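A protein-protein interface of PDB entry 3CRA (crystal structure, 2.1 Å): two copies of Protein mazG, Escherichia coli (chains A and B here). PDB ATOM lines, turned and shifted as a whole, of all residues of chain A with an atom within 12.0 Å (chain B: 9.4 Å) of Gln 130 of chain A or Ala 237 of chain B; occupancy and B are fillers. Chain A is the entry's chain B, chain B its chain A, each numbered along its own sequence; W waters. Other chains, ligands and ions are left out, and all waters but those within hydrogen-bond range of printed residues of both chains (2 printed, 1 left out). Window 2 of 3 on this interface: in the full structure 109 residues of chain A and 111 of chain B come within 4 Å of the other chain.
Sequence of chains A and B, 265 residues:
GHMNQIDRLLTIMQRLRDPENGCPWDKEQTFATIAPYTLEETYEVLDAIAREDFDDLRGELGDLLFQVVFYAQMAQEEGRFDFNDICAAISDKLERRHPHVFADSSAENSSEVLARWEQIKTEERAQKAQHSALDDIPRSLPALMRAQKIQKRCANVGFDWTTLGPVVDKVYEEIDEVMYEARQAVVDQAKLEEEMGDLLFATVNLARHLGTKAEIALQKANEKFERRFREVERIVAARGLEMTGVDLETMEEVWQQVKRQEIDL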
ATOM      1  N   GLN A 127       0.847  26.805   5.391  1.00  0.00           N
ATOM      2  CA  GLN A 127       1.562  27.943   4.825  1.00  0.00           C
ATOM      3  C   GLN A 127       2.962  27.546   4.373  1.00  0.00           C
ATOM      4  O   GLN A 127       3.825  27.025   5.112  1.00  0.00           O
ATOM      5  CB  GLN A 127       1.640  29.083   5.842  1.00  0.00           C
ATOM      6  CG  GLN A 127       0.300  29.724   6.161  1.00  0.00           C
ATOM      7  CD  GLN A 127       0.407  30.809   7.213  1.00  0.00           C
ATOM      8  OE1 GLN A 127       1.493  31.078   7.729  1.00  0.00           O
ATOM      9  NE2 GLN A 127      -0.719  31.439   7.534  1.00  0.00           N
ATOM     10  N   LYS A 128       3.271  27.905   3.077  1.00  0.00           N
ATOM     11  CA  LYS A 128       4.483  27.478   2.390  1.00  0.00           C
ATOM     12  C   LYS A 128       5.706  28.010   3.139  1.00  0.00           C
ATOM     13  O   LYS A 128       5.688  29.132   3.640  1.00  0.00           O
ATOM     14  CB  LYS A 128       4.479  27.950   0.908  1.00  0.00           C
ATOM     15  CG  LYS A 128       4.401  26.795  -0.147  1.00  0.00           C
ATOM     16  CD  LYS A 128       5.150  27.101  -1.447  1.00  0.00           C
ATOM     17  CE  LYS A 128       6.506  26.323  -1.596  1.00  0.00           C
ATOM     18  NZ  LYS A 128       7.322  26.637  -2.870  1.00  0.00           N
ATOM     19  N   ALA A 129       6.745  27.184   3.261  1.00  0.00           N
ATOM     20  CA  ALA A 129       8.084  27.703   3.553  1.00  0.00           C
ATOM     21  C   ALA A 129       8.698  28.219   2.230  1.00  0.00           C
ATOM     22  O   ALA A 129       8.191  27.922   1.130  1.00  0.00           O
ATOM     23  CB  ALA A 129       8.947  26.619   4.203  1.00  0.00           C
ATOM     24  N   GLN A 130       9.735  29.039   2.312  1.00  0.00           N
ATOM     25  CA  GLN A 130      10.513  29.310   1.123  1.00  0.00           C
ATOM     26  C   GLN A 130      10.966  27.961   0.453  1.00  0.00           C
ATOM     27  O   GLN A 130      11.371  27.020   1.125  1.00  0.00           O
ATOM     28  CB  GLN A 130      11.710  30.211   1.488  1.00  0.00           C
ATOM     29  CG  GLN A 130      12.641  30.632   0.311  1.00  0.00           C
ATOM     30  CD  GLN A 130      11.913  31.365  -0.836  1.00  0.00           C
ATOM     31  OE1 GLN A 130      12.232  31.181  -2.013  1.00  0.00           O
ATOM     32  NE2 GLN A 130      10.922  32.172  -0.485  1.00  0.00           N
ATOM     33  N   HIS A 131      10.839  27.867  -0.863  1.00  0.00           N
ATOM     34  CA  HIS A 131      11.283  26.715  -1.578  1.00  0.00           C
ATOM     35  C   HIS A 131      12.824  26.590  -1.520  1.00  0.00           C
ATOM     36  O   HIS A 131      13.524  27.608  -1.439  1.00  0.00           O
ATOM     37  CB  HIS A 131      10.723  26.745  -3.015  1.00  0.00           C
ATOM     38  CG  HIS A 131      11.609  27.405  -4.025  1.00  0.00           C
ATOM     39  ND1 HIS A 131      11.379  28.678  -4.496  1.00  0.00           N
ATOM     40  CD2 HIS A 131      12.708  26.959  -4.667  1.00  0.00           C
ATOM     41  CE1 HIS A 131      12.306  28.994  -5.382  1.00  0.00           C
ATOM     42  NE2 HIS A 131      13.123  27.964  -5.508  1.00  0.00           N
ATOM     43  N   SER A 132      13.325  25.348  -1.561  1.00  0.00           N
ATOM     44  CA  SER A 132      14.762  25.097  -1.409  1.00  0.00           C
ATOM     45  C   SER A 132      15.327  23.908  -2.140  1.00  0.00           C
ATOM     46  O   SER A 132      14.697  22.851  -2.227  1.00  0.00           O
ATOM     47  CB  SER A 132      15.105  24.905   0.063  1.00  0.00           C
ATOM     48  OG  SER A 132      16.508  24.885   0.164  1.00  0.00           O
ATOM     49  N   ALA A 133      16.583  24.048  -2.590  1.00  0.00           N
ATOM     50  CA  ALA A 133      17.281  22.948  -3.185  1.00  0.00           C
ATOM     51  C   ALA A 133      17.658  21.925  -2.111  1.00  0.00           C
ATOM     52  O   ALA A 133      18.094  20.806  -2.440  1.00  0.00           O
ATOM     53  CB  ALA A 133      18.570  23.459  -4.031  1.00  0.00           C
ATOM     54  N   LEU A 134      17.450  22.290  -0.845  1.00  0.00           N
ATOM     55  CA  LEU A 134      17.970  21.510   0.303  1.00  0.00           C
ATOM     56  C   LEU A 134      16.853  20.603   0.904  1.00  0.00           C
ATOM     57  O   LEU A 134      17.057  19.857   1.878  1.00  0.00           O
ATOM     58  CB  LEU A 134      18.608  22.430   1.374  1.00  0.00           C
ATOM     59  CG  LEU A 134      19.940  23.122   0.903  1.00  0.00           C
ATOM     60  CD1 LEU A 134      20.707  23.827   1.984  1.00  0.00           C
ATOM     61  CD2 LEU A 134      20.887  22.191   0.217  1.00  0.00           C
ATOM     62  N   ASP A 135      15.663  20.683   0.320  1.00  0.00           N
ATOM     63  CA  ASP A 135      14.552  19.944   0.882  1.00  0.00           C
ATOM     64  C   ASP A 135      14.715  18.469   0.772  1.00  0.00           C
ATOM     65  O   ASP A 135      15.408  18.005  -0.108  1.00  0.00           O
ATOM     66  CB  ASP A 135      13.257  20.423   0.260  1.00  0.00           C
ATOM     67  CG  ASP A 135      12.836  21.712   0.834  1.00  0.00           C
ATOM     68  OD1 ASP A 135      13.360  22.124   1.926  1.00  0.00           O
ATOM     69  OD2 ASP A 135      12.044  22.336   0.164  1.00  0.00           O
ATOM     70  N   ASP A 136      14.057  17.723   1.657  1.00  0.00           N
ATOM     71  CA  ASP A 136      14.138  16.255   1.662  1.00  0.00           C
ATOM     72  C   ASP A 136      15.525  15.700   1.842  1.00  0.00           C
ATOM     73  O   ASP A 136      15.988  14.880   1.035  1.00  0.00           O
ATOM     74  CB  ASP A 136      13.593  15.672   0.377  1.00  0.00           C
ATOM     75  CG  ASP A 136      13.307  14.177   0.511  1.00  0.00           C
ATOM     76  OD1 ASP A 136      12.844  13.892   1.603  1.00  0.00           O
ATOM     77  OD2 ASP A 136      13.599  13.315  -0.392  1.00  0.00           O
ATOM     78  N   ARG A 153      23.330  19.241  -3.744  1.00  0.00           N
ATOM     79  CA  ARG A 153      22.185  20.018  -4.067  1.00  0.00           C
ATOM     80  C   ARG A 153      22.717  21.366  -4.513  1.00  0.00           C
ATOM     81  O   ARG A 153      22.227  21.931  -5.501  1.00  0.00           O
ATOM     82  CB  ARG A 153      21.281  20.216  -2.828  1.00  0.00           C
ATOM     83  CG  ARG A 153      20.524  18.951  -2.352  1.00  0.00           C
ATOM     84  CD  ARG A 153      19.787  18.147  -3.482  1.00  0.00           C
ATOM     85  NE  ARG A 153      19.140  16.951  -2.850  1.00  0.00           N
ATOM     86  CZ  ARG A 153      18.068  17.068  -2.049  1.00  0.00           C
ATOM     87  NH1 ARG A 153      17.470  18.259  -1.906  1.00  0.00           N
ATOM     88  NH2 ARG A 153      17.524  16.004  -1.496  1.00  0.00           N
ATOM     89  N   VAL A 157      22.647  23.376  -8.619  1.00  0.00           N
ATOM     90  CA  VAL A 157      22.123  24.713  -8.784  1.00  0.00           C
ATOM     91  C   VAL A 157      23.260  25.760  -9.056  1.00  0.00           C
ATOM     92  O   VAL A 157      23.016  26.965  -9.112  1.00  0.00           O
ATOM     93  CB  VAL A 157      21.234  24.920  -7.527  1.00  0.00           C
ATOM     94  CG1 VAL A 157      21.630  25.947  -6.593  1.00  0.00           C
ATOM     95  CG2 VAL A 157      19.715  24.665  -7.755  1.00  0.00           C
ATOM     96  N   GLU B 226      23.370  25.013   5.808  1.00  0.00           N
ATOM     97  CA  GLU B 226      22.010  24.961   5.333  1.00  0.00           C
ATOM     98  C   GLU B 226      21.256  26.256   5.597  1.00  0.00           C
ATOM     99  O   GLU B 226      20.611  26.801   4.711  1.00  0.00           O
ATOM    100  CB  GLU B 226      21.359  23.743   6.003  1.00  0.00           C
ATOM    101  CG  GLU B 226      19.886  23.681   5.766  1.00  0.00           C
ATOM    102  CD  GLU B 226      19.384  22.298   5.539  1.00  0.00           C
ATOM    103  OE1 GLU B 226      20.009  21.286   5.930  1.00  0.00           O
ATOM    104  OE2 GLU B 226      18.304  22.256   4.992  1.00  0.00           O
ATOM    105  N   PHE B 229      22.595  28.861   3.301  1.00  0.00           N
ATOM    106  CA  PHE B 229      22.274  28.662   1.869  1.00  0.00           C
ATOM    107  C   PHE B 229      20.850  29.058   1.624  1.00  0.00           C
ATOM    108  O   PHE B 229      20.566  29.699   0.646  1.00  0.00           O
ATOM    109  CB  PHE B 229      22.527  27.208   1.370  1.00  0.00           C
ATOM    110  CG  PHE B 229      22.401  27.098  -0.079  1.00  0.00           C
ATOM    111  CD1 PHE B 229      23.399  27.623  -0.905  1.00  0.00           C
ATOM    112  CD2 PHE B 229      21.226  26.609  -0.654  1.00  0.00           C
ATOM    113  CE1 PHE B 229      23.266  27.591  -2.297  1.00  0.00           C
ATOM    114  CE2 PHE B 229      21.072  26.536  -2.065  1.00  0.00           C
ATOM    115  CZ  PHE B 229      22.067  27.005  -2.883  1.00  0.00           C
ATOM    116  N   ARG B 230      19.981  28.650   2.534  1.00  0.00           N
ATOM    117  CA  ARG B 230      18.568  28.977   2.547  1.00  0.00           C
ATOM    118  C   ARG B 230      18.342  30.505   2.484  1.00  0.00           C
ATOM    119  O   ARG B 230      17.537  31.002   1.675  1.00  0.00           O
ATOM    120  CB  ARG B 230      17.893  28.247   3.725  1.00  0.00           C
ATOM    121  CG  ARG B 230      17.712  26.716   3.383  1.00  0.00           C
ATOM    122  CD  ARG B 230      17.206  25.771   4.521  1.00  0.00           C
ATOM    123  NE  ARG B 230      15.891  25.350   4.092  1.00  0.00           N
ATOM    124  CZ  ARG B 230      15.463  24.143   3.753  1.00  0.00           C
ATOM    125  NH1 ARG B 230      16.152  23.042   3.868  1.00  0.00           N
ATOM    126  NH2 ARG B 230      14.242  24.069   3.332  1.00  0.00           N
ATOM    127  N   GLU B 231      19.124  31.254   3.253  1.00  0.00           N
ATOM    128  CA  GLU B 231      19.086  32.715   3.188  1.00  0.00           C
ATOM    129  C   GLU B 231      19.510  33.262   1.775  1.00  0.00           C
ATOM    130  O   GLU B 231      18.777  34.028   1.154  1.00  0.00           O
ATOM    131  CB  GLU B 231      19.916  33.314   4.344  1.00  0.00           C
ATOM    132  CG  GLU B 231      19.943  34.844   4.417  1.00  0.00           C
ATOM    133  CD  GLU B 231      18.583  35.500   4.738  1.00  0.00           C
ATOM    134  OE1 GLU B 231      18.604  36.756   4.733  1.00  0.00           O
ATOM    135  OE2 GLU B 231      17.526  34.811   4.962  1.00  0.00           O
ATOM    136  N   VAL B 232      20.658  32.865   1.262  1.00  0.00           N
ATOM    137  CA  VAL B 232      21.004  33.235  -0.087  1.00  0.00           C
ATOM    138  C   VAL B 232      19.841  32.911  -1.115  1.00  0.00           C
ATOM    139  O   VAL B 232      19.539  33.696  -2.080  1.00  0.00           O
ATOM    140  CB  VAL B 232      22.241  32.464  -0.496  1.00  0.00           C
ATOM    141  CG1 VAL B 232      22.623  32.804  -1.903  1.00  0.00           C
ATOM    142  CG2 VAL B 232      23.398  32.679   0.491  1.00  0.00           C
ATOM    143  N   GLU B 233      19.231  31.729  -0.946  1.00  0.00           N
ATOM    144  CA  GLU B 233      18.103  31.323  -1.780  1.00  0.00           C
ATOM    145  C   GLU B 233      16.937  32.324  -1.670  1.00  0.00           C
ATOM    146  O   GLU B 233      16.366  32.733  -2.668  1.00  0.00           O
ATOM    147  CB  GLU B 233      17.605  29.958  -1.340  1.00  0.00           C
ATOM    148  CG  GLU B 233      18.403  28.814  -1.883  1.00  0.00           C
ATOM    149  CD  GLU B 233      17.809  27.471  -1.501  1.00  0.00           C
ATOM    150  OE1 GLU B 233      17.348  27.279  -0.352  1.00  0.00           O
ATOM    151  OE2 GLU B 233      17.786  26.615  -2.384  1.00  0.00           O
ATOM    152  N   ARG B 234      16.565  32.638  -0.438  1.00  0.00           N
ATOM    153  CA  ARG B 234      15.538  33.634  -0.086  1.00  0.00           C
ATOM    154  C   ARG B 234      15.875  34.983  -0.717  1.00  0.00           C
ATOM    155  O   ARG B 234      15.019  35.630  -1.300  1.00  0.00           O
ATOM    156  CB  ARG B 234      15.501  33.796   1.429  1.00  0.00           C
ATOM    157  CG  ARG B 234      14.400  34.720   1.938  1.00  0.00           C
ATOM    158  CD  ARG B 234      14.956  35.646   3.038  1.00  0.00           C
ATOM    159  NE  ARG B 234      14.578  37.027   2.722  1.00  0.00           N
ATOM    160  CZ  ARG B 234      15.377  38.103   2.747  1.00  0.00           C
ATOM    161  NH1 ARG B 234      16.649  38.017   3.136  1.00  0.00           N
ATOM    162  NH2 ARG B 234      14.872  39.294   2.403  1.00  0.00           N
ATOM    163  N   ILE B 235      17.135  35.392  -0.611  1.00  0.00           N
ATOM    164  CA  ILE B 235      17.575  36.648  -1.193  1.00  0.00           C
ATOM    165  C   ILE B 235      17.513  36.605  -2.723  1.00  0.00           C
ATOM    166  O   ILE B 235      16.847  37.453  -3.338  1.00  0.00           O
ATOM    167  CB  ILE B 235      18.987  37.088  -0.699  1.00  0.00           C
ATOM    168  CG1 ILE B 235      19.004  37.382   0.813  1.00  0.00           C
ATOM    169  CG2 ILE B 235      19.454  38.321  -1.450  1.00  0.00           C
ATOM    170  CD1 ILE B 235      20.433  37.777   1.319  1.00  0.00           C
ATOM    171  N   VAL B 236      18.198  35.658  -3.358  1.00  0.00           N
ATOM    172  CA  VAL B 236      18.146  35.572  -4.823  1.00  0.00           C
ATOM    173  C   VAL B 236      16.690  35.486  -5.309  1.00  0.00           C
ATOM    174  O   VAL B 236      16.350  36.030  -6.351  1.00  0.00           O
ATOM    175  CB  VAL B 236      18.956  34.348  -5.357  1.00  0.00           C
ATOM    176  CG1 VAL B 236      18.558  33.998  -6.826  1.00  0.00           C
ATOM    177  CG2 VAL B 236      20.460  34.593  -5.232  1.00  0.00           C
ATOM    178  N   ALA B 237      15.843  34.792  -4.551  1.00  0.00           N
ATOM    179  CA  ALA B 237      14.447  34.559  -4.927  1.00  0.00           C
ATOM    180  C   ALA B 237      13.594  35.835  -4.796  1.00  0.00           C
ATOM    181  O   ALA B 237      12.776  36.160  -5.670  1.00  0.00           O
ATOM    182  CB  ALA B 237      13.869  33.434  -4.114  1.00  0.00           C
ATOM    183  N   ALA B 238      13.805  36.577  -3.714  1.00  0.00           N
ATOM    184  CA  ALA B 238      13.107  37.827  -3.536  1.00  0.00           C
ATOM    185  C   ALA B 238      13.493  38.823  -4.632  1.00  0.00           C
ATOM    186  O   ALA B 238      12.764  39.775  -4.887  1.00  0.00           O
ATOM    187  CB  ALA B 238      13.399  38.396  -2.156  1.00  0.00           C
ATOM    188  N   ARG B 239      14.606  38.583  -5.318  1.00  0.00           N
ATOM    189  CA  ARG B 239      15.175  39.636  -6.166  1.00  0.00           C
ATOM    190  C   ARG B 239      14.189  40.440  -7.000  1.00  0.00           C
ATOM    191  O   ARG B 239      14.116  41.660  -6.779  1.00  0.00           O
ATOM    192  CB  ARG B 239      16.475  39.269  -6.893  1.00  0.00           C
ATOM    193  CG  ARG B 239      17.577  40.142  -6.381  1.00  0.00           C
ATOM    194  CD  ARG B 239      18.746  39.355  -5.863  1.00  0.00           C
ATOM    195  NE  ARG B 239      19.505  40.095  -4.837  1.00  0.00           N
ATOM    196  CZ  ARG B 239      20.792  40.450  -4.940  1.00  0.00           C
ATOM    197  NH1 ARG B 239      21.498  40.160  -6.042  1.00  0.00           N
ATOM    198  NH2 ARG B 239      21.380  41.103  -3.928  1.00  0.00           N
ATOM    199  N   GLY B 240      13.410  39.814  -7.900  1.00  0.00           N
ATOM    200  CA  GLY B 240      13.325  38.375  -8.042  1.00  0.00           C
ATOM    201  C   GLY B 240      13.304  37.939  -9.492  1.00  0.00           C
ATOM    202  O   GLY B 240      14.358  37.866 -10.150  1.00  0.00           O
ATOM    203  N   LEU B 241      12.134  37.609  -9.981  1.00  0.00           N
ATOM    204  CA  LEU B 241      11.865  37.189 -11.352  1.00  0.00           C
ATOM    205  C   LEU B 241      12.981  36.301 -11.887  1.00  0.00           C
ATOM    206  O   LEU B 241      12.874  35.041 -11.972  1.00  0.00           O
ATOM    207  CB  LEU B 241      11.682  38.408 -12.259  1.00  0.00           C
ATOM    208  CG  LEU B 241      10.473  39.299 -11.963  1.00  0.00           C
ATOM    209  CD1 LEU B 241      10.489  40.536 -12.847  1.00  0.00           C
ATOM    210  CD2 LEU B 241       9.177  38.524 -12.142  1.00  0.00           C
ATOM    211  N   GLU B 242      14.033  36.957 -12.353  1.00  0.00           N
ATOM    212  CA  GLU B 242      15.101  36.398 -13.163  1.00  0.00           C
ATOM    213  C   GLU B 242      15.033  34.923 -13.694  1.00  0.00           C
ATOM    214  O   GLU B 242      15.443  33.939 -13.055  1.00  0.00           O
ATOM    215  CB  GLU B 242      16.501  36.817 -12.628  1.00  0.00           C
ATOM    216  CG  GLU B 242      16.678  38.340 -12.228  1.00  0.00           C
ATOM    217  CD  GLU B 242      16.132  39.404 -13.263  1.00  0.00           C
ATOM    218  OE1 GLU B 242      14.899  39.445 -13.534  1.00  0.00           O
ATOM    219  OE2 GLU B 242      16.946  40.224 -13.772  1.00  0.00           O
ATOM    220  N   THR B 250      26.096  37.137  -9.354  1.00  0.00           N
ATOM    221  CA  THR B 250      25.268  36.548  -8.215  1.00  0.00           C
ATOM    222  C   THR B 250      25.865  35.917  -6.879  1.00  0.00           C
ATOM    223  O   THR B 250      26.084  36.640  -5.880  1.00  0.00           O
ATOM    224  CB  THR B 250      23.992  35.686  -8.769  1.00  0.00           C
ATOM    225  OG1 THR B 250      23.173  36.476  -9.650  1.00  0.00           O
ATOM    226  CG2 THR B 250      23.103  35.138  -7.637  1.00  0.00           C
ATOM    227  N   MET B 251      26.105  34.594  -6.881  1.00  0.00           N
ATOM    228  CA  MET B 251      25.981  33.744  -5.667  1.00  0.00           C
ATOM    229  C   MET B 251      27.017  33.849  -4.528  1.00  0.00           C
ATOM    230  O   MET B 251      26.634  33.853  -3.351  1.00  0.00           O
ATOM    231  CB  MET B 251      25.687  32.274  -6.036  1.00  0.00           C
ATOM    232  CG  MET B 251      24.163  32.004  -6.217  1.00  0.00           C
ATOM    233  SD  MET B 251      23.537  30.299  -6.374  1.00  0.00           S
ATOM    234  CE  MET B 251      24.540  29.637  -7.712  1.00  0.00           C
ATOM    235  N   VAL B 254      26.472  37.158  -2.424  1.00  0.00           N
ATOM    236  CA  VAL B 254      25.349  37.042  -1.468  1.00  0.00           C
ATOM    237  C   VAL B 254      25.740  36.106  -0.300  1.00  0.00           C
ATOM    238  O   VAL B 254      25.487  36.441   0.860  1.00  0.00           O
ATOM    239  CB  VAL B 254      23.979  36.630  -2.130  1.00  0.00           C
ATOM    240  CG1 VAL B 254      22.818  36.863  -1.156  1.00  0.00           C
ATOM    241  CG2 VAL B 254      23.735  37.396  -3.455  1.00  0.00           C
HETATM  242  O   HOH W   1      17.698  19.907   4.215  1.00  0.00           O
HETATM  243  O   HOH W   2      13.992  27.484   2.737  1.00  0.00           O
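CB of Ala 237 of chain B touches OE1 of Gln 130 of chain A, 3.5 Å away. His 131 of chain A touches Glu 233 of chain B. CB of Ser 132 of chain A touches NH2 of Arg 230 of chain B (3.5 Å). Leu 134 of chain A touches Glu 226 of chain B (CB to OE2, 3.6 Å). Leu 134 of chain A touches Phe 229 of chain B. Arg 230 of chain B touches Leu 134 of chain A. Phe 229 of chain B touches Val 157 of chain A. Met 251 of chain B touches Val 157 of chain A (CE to O, 3.4 Å).
Water W1 lies within hydrogen-bond range of the backbone carbonyl oxygen of Leu 134 of chain A (2.4 Å) and the side-chain carboxylate of Glu 226 of chain B (2.5 Å). Water W2 lies within hydrogen-bond range of O of Gln 130 of chain A (3.1 Å) and NE of Arg 230 of chain B (3.2 Å).
OE2 of Glu 233 of chain B is in hydrogen-bond range of N of Ala 133 of chain A (2.8 Å). The side-chain carboxylate (OE1) of Glu 233 of chain B lies within hydrogen-bond range of the side-chain hydroxyl (OG) of Ser 132 of chain A (2.6 Å). The guanidinium group (NH2) of Arg 230 of chain B lies within salt-bridge range of the side-chain carboxylate (OD1) of Asp 135 of chain A, 2.6 Å away.
Of the 12 printed residues of chain A, 7 touch a printed residue of chain B. Printed residues of chain A that touch a printed residue of chain B: Gln 130, His 131, Ser 132, Ala 133, Leu 134, Asp 135 and Val 157. Hydrophobic or aromatic side chains of chain A that line the printed part of chain B: Ala 133, Leu 134 and Val 157. Along chain A the printed residues that touch a printed residue of chain B span positions 130 to 157. Printed residues of chain B that touch a printed residue of chain A: Glu 226, Phe 229, Arg 230, Glu 233, Ala 237 and Met 251. Hydrophobic or aromatic side chains of chain B that line the printed part of chain A: Phe 229, Ala 237 and Met 251. Along chain B the printed residues that touch a printed residue of chain A span positions 226 to 251. Among the printed residues, 11 pairs touch across the chains. Among the printed residues, Asp or Glu carboxylates within 4 Å of a Lys or Arg side-chain nitrogen of the other chain: Asp 135 of chain A with Arg 230 of chain B (2.6 Å).
The backbone carbonyl oxygen of Asp 135 of chain A is in hydrogen-bond range of the guanidinium group of Arg 153 of chain A (2.7 Å). The backbone NH of Leu 134 of chain A lies within hydrogen-bond range of the side-chain hydroxyl of Ser 132 of chain A, 2.9 Å away. OE2 of Glu 226 of chain B is in salt-bridge range of NH1 of Arg 230 of chain B, at 2.6 Å. NH1 of Arg 153 of chain A sits at hydrogen-bond distance from O of Ala 133 of chain A (2.7 Å).
No position is printed for both chains. Of the 11 pairs that touch across the chains among the printed residues, none has its exchanged pair printed and touching as well.
Of chain B, only Ala 237 comes within 4 Å of Gln 130 of chain A. Printed residues of chain A within 4 Å of Ala 237 of chain B: Gln 130. No residue of chain A comes within 4 Å of Ala 238 of chain B. Printed residues of chain B within 4 Å of Ser 132 of chain A: Arg 230 (3.5 Å) and Glu 233 (2.6 Å). Of the printed residues of chain B, His 131 of chain A touches Glu 233 (3.99 Å). Printed residues of chain A within 4 Å of Phe 229 of chain B: Leu 134 (3.9 Å) and Val 157 (3.9 Å). Of the printed residues of chain B, Val 157 of chain A touches Phe 229 (3.9 Å) and Met 251 (3.4 Å). Printed residues of chain B within 4 Å of Ala 133 of chain A: Glu 233. The nearest residue of chain B that does not touch Gln 130 of chain A is Arg 234 of chain B (4.2 Å). The nearest residue of chain A that does not touch Ala 237 of chain B is His 131 of chain A (4.9 Å). The nearest printed residue of chain B that does not touch His 131 of chain A is Ala 237 of chain B (4.9 Å).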
